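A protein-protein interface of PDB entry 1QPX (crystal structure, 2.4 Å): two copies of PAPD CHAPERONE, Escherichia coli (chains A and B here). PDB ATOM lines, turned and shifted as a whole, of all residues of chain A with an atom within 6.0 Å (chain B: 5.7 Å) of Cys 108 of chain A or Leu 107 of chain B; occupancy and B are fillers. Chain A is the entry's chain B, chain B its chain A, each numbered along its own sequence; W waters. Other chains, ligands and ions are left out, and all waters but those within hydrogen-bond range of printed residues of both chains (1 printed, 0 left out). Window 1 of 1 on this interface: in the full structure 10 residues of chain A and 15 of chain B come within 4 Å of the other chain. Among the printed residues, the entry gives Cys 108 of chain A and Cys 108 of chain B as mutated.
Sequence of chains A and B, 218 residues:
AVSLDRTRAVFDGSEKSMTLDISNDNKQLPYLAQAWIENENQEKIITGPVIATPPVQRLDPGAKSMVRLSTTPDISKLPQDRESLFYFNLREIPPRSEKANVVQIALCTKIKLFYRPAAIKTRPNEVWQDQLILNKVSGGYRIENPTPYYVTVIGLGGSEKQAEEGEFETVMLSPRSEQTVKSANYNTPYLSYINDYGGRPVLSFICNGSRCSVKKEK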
ATOM      1  N   LEU A  90      16.421  16.951 -27.369  1.00  0.00           N
ATOM      2  CA  LEU A  90      15.284  17.875 -27.357  1.00  0.00           C
ATOM      3  C   LEU A  90      15.761  19.309 -27.102  1.00  0.00           C
ATOM      4  O   LEU A  90      16.453  19.604 -26.139  1.00  0.00           O
ATOM      5  CB  LEU A  90      14.208  17.531 -26.342  1.00  0.00           C
ATOM      6  CG  LEU A  90      12.880  18.308 -26.525  1.00  0.00           C
ATOM      7  CD1 LEU A  90      12.210  17.820 -27.806  1.00  0.00           C
ATOM      8  CD2 LEU A  90      12.014  18.134 -25.282  1.00  0.00           C
ATOM      9  N   ARG A  91      15.376  20.227 -27.965  1.00  0.00           N
ATOM     10  CA  ARG A  91      15.782  21.606 -27.752  1.00  0.00           C
ATOM     11  C   ARG A  91      14.550  22.517 -27.767  1.00  0.00           C
ATOM     12  O   ARG A  91      13.742  22.473 -28.689  1.00  0.00           O
ATOM     13  CB  ARG A  91      16.803  21.977 -28.782  1.00  0.00           C
ATOM     14  CG  ARG A  91      17.556  23.249 -28.501  1.00  0.00           C
ATOM     15  CD  ARG A  91      18.686  23.358 -29.541  1.00  0.00           C
ATOM     16  NE  ARG A  91      18.495  24.645 -30.206  1.00  0.00           N
ATOM     17  CZ  ARG A  91      19.359  25.646 -29.992  1.00  0.00           C
ATOM     18  NH1 ARG A  91      20.390  25.254 -29.221  1.00  0.00           N
ATOM     19  NH2 ARG A  91      19.132  26.829 -30.541  1.00  0.00           N
ATOM     20  N   GLU A  92      14.418  23.336 -26.753  1.00  0.00           N
ATOM     21  CA  GLU A  92      13.252  24.238 -26.739  1.00  0.00           C
ATOM     22  C   GLU A  92      13.713  25.678 -26.804  1.00  0.00           C
ATOM     23  O   GLU A  92      14.528  26.075 -25.953  1.00  0.00           O
ATOM     24  CB  GLU A  92      12.404  23.985 -25.489  1.00  0.00           C
ATOM     25  CG  GLU A  92      11.767  22.625 -25.388  1.00  0.00           C
ATOM     26  CD  GLU A  92      11.095  22.308 -24.060  1.00  0.00           C
ATOM     27  OE1 GLU A  92      10.493  23.227 -23.425  1.00  0.00           O
ATOM     28  OE2 GLU A  92      11.156  21.143 -23.638  1.00  0.00           O
ATOM     29  N   ILE A 105      19.282  31.558 -26.172  1.00  0.00           N
ATOM     30  CA  ILE A 105      19.277  30.690 -25.004  1.00  0.00           C
ATOM     31  C   ILE A 105      18.096  29.711 -25.089  1.00  0.00           C
ATOM     32  O   ILE A 105      16.920  30.072 -25.200  1.00  0.00           O
ATOM     33  CB  ILE A 105      19.230  31.435 -23.664  1.00  0.00           C
ATOM     34  CG1 ILE A 105      20.455  32.335 -23.519  1.00  0.00           C
ATOM     35  CG2 ILE A 105      19.111  30.448 -22.508  1.00  0.00           C
ATOM     36  CD1 ILE A 105      20.471  33.052 -22.178  1.00  0.00           C
ATOM     37  N   ALA A 106      18.414  28.422 -25.025  1.00  0.00           N
ATOM     38  CA  ALA A 106      17.440  27.374 -25.190  1.00  0.00           C
ATOM     39  C   ALA A 106      17.573  26.304 -24.130  1.00  0.00           C
ATOM     40  O   ALA A 106      18.613  26.154 -23.475  1.00  0.00           O
ATOM     41  CB  ALA A 106      17.674  26.726 -26.572  1.00  0.00           C
ATOM     42  N   LEU A 107      16.514  25.509 -23.966  1.00  0.00           N
ATOM     43  CA  LEU A 107      16.569  24.352 -23.056  1.00  0.00           C
ATOM     44  C   LEU A 107      16.957  23.146 -23.897  1.00  0.00           C
ATOM     45  O   LEU A 107      16.378  22.948 -24.973  1.00  0.00           O
ATOM     46  CB  LEU A 107      15.247  24.072 -22.339  1.00  0.00           C
ATOM     47  CG  LEU A 107      14.727  25.434 -21.761  1.00  0.00           C
ATOM     48  CD1 LEU A 107      13.255  25.442 -21.427  1.00  0.00           C
ATOM     49  CD2 LEU A 107      15.587  25.773 -20.534  1.00  0.00           C
ATOM     50  N   CYS A 108      17.981  22.427 -23.471  1.00  0.00           N
ATOM     51  CA  CYS A 108      18.424  21.313 -24.333  1.00  0.00           C
ATOM     52  C   CYS A 108      18.534  20.079 -23.464  1.00  0.00           C
ATOM     53  O   CYS A 108      19.017  20.106 -22.326  1.00  0.00           O
ATOM     54  CB  CYS A 108      19.625  21.764 -25.197  1.00  0.00           C
ATOM     55  SG  CYS A 108      20.850  22.554 -24.090  1.00  0.00           S
ATOM     56  N   THR A 109      17.942  18.976 -23.899  1.00  0.00           N
ATOM     57  CA  THR A 109      17.995  17.726 -23.181  1.00  0.00           C
ATOM     58  C   THR A 109      18.576  16.660 -24.118  1.00  0.00           C
ATOM     59  O   THR A 109      18.267  16.644 -25.327  1.00  0.00           O
ATOM     60  CB  THR A 109      16.586  17.265 -22.763  1.00  0.00           C
ATOM     61  OG1 THR A 109      16.033  18.168 -21.804  1.00  0.00           O
ATOM     62  CG2 THR A 109      16.556  15.928 -22.046  1.00  0.00           C
ATOM     63  N   LYS A 110      19.320  15.750 -23.479  1.00  0.00           N
ATOM     64  CA  LYS A 110      19.749  14.603 -24.296  1.00  0.00           C
ATOM     65  C   LYS A 110      19.659  13.349 -23.465  1.00  0.00           C
ATOM     66  O   LYS A 110      20.190  13.273 -22.368  1.00  0.00           O
ATOM     67  CB  LYS A 110      21.005  14.850 -25.060  1.00  0.00           C
ATOM     68  CG  LYS A 110      22.327  14.729 -24.420  1.00  0.00           C
ATOM     69  CD  LYS A 110      23.261  15.632 -25.249  1.00  0.00           C
ATOM     70  CE  LYS A 110      23.728  14.993 -26.524  1.00  0.00           C
ATOM     71  NZ  LYS A 110      24.420  15.962 -27.423  1.00  0.00           N
ATOM     72  N   ALA B   1      24.227  28.191 -13.480  1.00  0.00           N
ATOM     73  CA  ALA B   1      23.905  28.764 -14.815  1.00  0.00           C
ATOM     74  C   ALA B   1      25.199  29.505 -15.204  1.00  0.00           C
ATOM     75  O   ALA B   1      25.723  30.372 -14.509  1.00  0.00           O
ATOM     76  CB  ALA B   1      22.630  29.510 -15.001  1.00  0.00           C
ATOM     77  N   LEU B  90      27.689  26.714 -26.113  1.00  0.00           N
ATOM     78  CA  LEU B  90      27.980  26.412 -24.720  1.00  0.00           C
ATOM     79  C   LEU B  90      26.790  25.706 -24.121  1.00  0.00           C
ATOM     80  O   LEU B  90      25.654  26.143 -24.315  1.00  0.00           O
ATOM     81  CB  LEU B  90      28.254  27.723 -23.967  1.00  0.00           C
ATOM     82  CG  LEU B  90      28.752  27.499 -22.538  1.00  0.00           C
ATOM     83  CD1 LEU B  90      30.199  27.007 -22.523  1.00  0.00           C
ATOM     84  CD2 LEU B  90      28.681  28.857 -21.845  1.00  0.00           C
ATOM     85  N   ARG B  91      27.026  24.578 -23.468  1.00  0.00           N
ATOM     86  CA  ARG B  91      25.907  23.819 -22.880  1.00  0.00           C
ATOM     87  C   ARG B  91      26.262  23.645 -21.402  1.00  0.00           C
ATOM     88  O   ARG B  91      27.338  23.143 -21.106  1.00  0.00           O
ATOM     89  CB  ARG B  91      25.739  22.463 -23.551  1.00  0.00           C
ATOM     90  CG  ARG B  91      24.827  21.468 -22.830  1.00  0.00           C
ATOM     91  CD  ARG B  91      24.255  20.414 -23.804  1.00  0.00           C
ATOM     92  NE  ARG B  91      24.510  19.117 -23.205  1.00  0.00           N
ATOM     93  CZ  ARG B  91      23.573  18.417 -22.549  1.00  0.00           C
ATOM     94  NH1 ARG B  91      22.308  18.838 -22.451  1.00  0.00           N
ATOM     95  NH2 ARG B  91      23.859  17.253 -21.961  1.00  0.00           N
ATOM     96  N   GLU B  92      25.341  23.974 -20.536  1.00  0.00           N
ATOM     97  CA  GLU B  92      25.638  23.777 -19.114  1.00  0.00           C
ATOM     98  C   GLU B  92      24.985  22.495 -18.636  1.00  0.00           C
ATOM     99  O   GLU B  92      23.866  22.240 -19.009  1.00  0.00           O
ATOM    100  CB  GLU B  92      25.137  24.977 -18.323  1.00  0.00           C
ATOM    101  CG  GLU B  92      23.637  24.987 -18.107  1.00  0.00           C
ATOM    102  CD  GLU B  92      23.180  26.129 -17.198  1.00  0.00           C
ATOM    103  OE1 GLU B  92      22.371  25.783 -16.303  1.00  0.00           O
ATOM    104  OE2 GLU B  92      23.620  27.271 -17.354  1.00  0.00           O
ATOM    105  N   ILE B 105      17.796  18.928 -17.400  1.00  0.00           N
ATOM    106  CA  ILE B 105      17.337  20.210 -17.975  1.00  0.00           C
ATOM    107  C   ILE B 105      18.402  21.306 -18.032  1.00  0.00           C
ATOM    108  O   ILE B 105      18.426  22.313 -17.333  1.00  0.00           O
ATOM    109  CB  ILE B 105      16.083  20.697 -17.237  1.00  0.00           C
ATOM    110  CG1 ILE B 105      15.573  22.040 -17.772  1.00  0.00           C
ATOM    111  CG2 ILE B 105      16.347  20.711 -15.733  1.00  0.00           C
ATOM    112  CD1 ILE B 105      14.056  22.131 -17.707  1.00  0.00           C
ATOM    113  N   ALA B 106      19.345  21.132 -18.952  1.00  0.00           N
ATOM    114  CA  ALA B 106      20.462  21.978 -19.279  1.00  0.00           C
ATOM    115  C   ALA B 106      20.041  23.201 -20.092  1.00  0.00           C
ATOM    116  O   ALA B 106      18.949  23.278 -20.663  1.00  0.00           O
ATOM    117  CB  ALA B 106      21.454  21.121 -20.103  1.00  0.00           C
ATOM    118  N   LEU B 107      20.915  24.190 -20.150  1.00  0.00           N
ATOM    119  CA  LEU B 107      20.774  25.413 -20.878  1.00  0.00           C
ATOM    120  C   LEU B 107      21.883  25.459 -21.962  1.00  0.00           C
ATOM    121  O   LEU B 107      23.025  25.113 -21.652  1.00  0.00           O
ATOM    122  CB  LEU B 107      20.905  26.647 -20.014  1.00  0.00           C
ATOM    123  CG  LEU B 107      19.860  26.979 -18.965  1.00  0.00           C
ATOM    124  CD1 LEU B 107      19.895  28.471 -18.628  1.00  0.00           C
ATOM    125  CD2 LEU B 107      18.460  26.563 -19.366  1.00  0.00           C
ATOM    126  N   CYS B 108      21.476  25.930 -23.126  1.00  0.00           N
ATOM    127  CA  CYS B 108      22.382  25.989 -24.270  1.00  0.00           C
ATOM    128  C   CYS B 108      22.355  27.440 -24.804  1.00  0.00           C
ATOM    129  O   CYS B 108      21.291  28.000 -25.061  1.00  0.00           O
ATOM    130  CB  CYS B 108      21.977  25.040 -25.400  1.00  0.00           C
ATOM    131  SG  CYS B 108      22.309  23.252 -25.277  1.00  0.00           S
ATOM    132  N   THR B 109      23.534  28.005 -24.964  1.00  0.00           N
ATOM    133  CA  THR B 109      23.765  29.342 -25.464  1.00  0.00           C
ATOM    134  C   THR B 109      24.547  29.197 -26.784  1.00  0.00           C
ATOM    135  O   THR B 109      25.480  28.373 -26.906  1.00  0.00           O
ATOM    136  CB  THR B 109      24.685  30.111 -24.489  1.00  0.00           C
ATOM    137  OG1 THR B 109      24.065  30.009 -23.209  1.00  0.00           O
ATOM    138  CG2 THR B 109      24.897  31.561 -24.852  1.00  0.00           C
HETATM  139  O   HOH W   1      21.335  27.352 -28.302  1.00  0.00           O
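O of Cys 108 of chain B touches CA of Ile 105 of chain A, 3.4 Å away.
CA of Leu 107 of chain B touches O of Ala 106 of chain A (3.5 Å).
Leu 107 of chain A touches Ala 106 of chain B.
Leu 107 of chain B touches Leu 107 of chain A.
Cys 108 of chain A touches Arg 91 of chain B.
Leu 107 of chain B touches Cys 108 of chain A (C to SG, 3.7 Å).
CD of Lys 110 of chain A touches NH2 of Arg 91 of chain B, 3.7 Å away.
The backbone NH of Cys 108 of chain B sits at hydrogen-bond distance from the backbone carbonyl oxygen of Ala 106 of chain A.
The side-chain sulfur (SG) of Cys 108 of chain B is disulfide-bonded to the side-chain sulfur (SG) of Cys 108 of chain A (2.0 Å).
N of Cys 108 of chain A is in hydrogen-bond range of O of Ala 106 of chain B, 3.1 Å away.
Water W1 bridges NH1 of Arg 91 of chain A (2.5 Å) and O of Cys 108 of chain B (3.3 Å).
Printed residues of chain B that touch a printed residue of chain A: Arg 91, Ala 106, Leu 107 and Cys 108.
Hydrophobic or aromatic side chains of chain B within 4 Å of the printed part of chain A: Ala 106 and Leu 107.
Along chain B the printed residues that touch a printed residue of chain A span positions 91 to 108.
Of the 9 printed residues of chain A, 5 touch a printed residue of chain B.
Printed residues of chain A that touch a printed residue of chain B: Ile 105, Ala 106, Leu 107, Cys 108 and Lys 110.
Hydrophobic or aromatic side chains of chain A that line the printed part of chain B: Leu 107.
Along chain A the printed residues that touch a printed residue of chain B span positions 105 to 110.
Among the printed residues, 10 pairs touch across the chains.
Among the printed residues, no Asp or Glu carboxylate lies within 4 Å of a Lys or Arg side-chain nitrogen of the other chain.
Ile 105 of chain A touches Cys 108 of chain B, but with the chains exchanged Cys 108 of chain A does not touch Ile 105 of chain B (4.5 Å).
Ala 106 of chain A touches Leu 107 of chain B, and with the chains exchanged Leu 107 of chain A touches Ala 106 of chain B.
Ala 106 of chain A touches Cys 108 of chain B, and with the chains exchanged Cys 108 of chain A touches Ala 106 of chain B.
Cys 108 of chain A touches its own counterpart, Cys 108 of chain B.
Positions printed for both chains: 90, 91, 92, 105, 106, 107, 108 and 109.
The backbone NH (N) of Glu 92 of chain A sits at hydrogen-bond distance from the backbone carbonyl oxygen (O) of Leu 107 of chain A, 2.7 Å away.
The backbone NH (N) of Glu 92 of chain B sits at hydrogen-bond distance from the backbone carbonyl oxygen (O) of Leu 107 of chain B (2.8 Å).
Of the printed residues of chain B, Ile 105 of chain A touches Cys 108.
Of the printed residues of chain B, Lys 110 of chain A touches Arg 91.
Glu 92 of chain B touches none of the printed residues of chain A.
Leu 107 of chain B touches three residues of chain A.
The nearest residue of chain B that does not touch Cys 108 of chain A is Ile 105 of chain B (4.5 Å).
The nearest residue of chain A that does not touch Leu 107 of chain B is Ile 105 of chain A (4.4 Å).
The nearest printed residue of chain A that does not touch Ala 106 of chain B is Ala 106 of chain A (4.04 Å).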
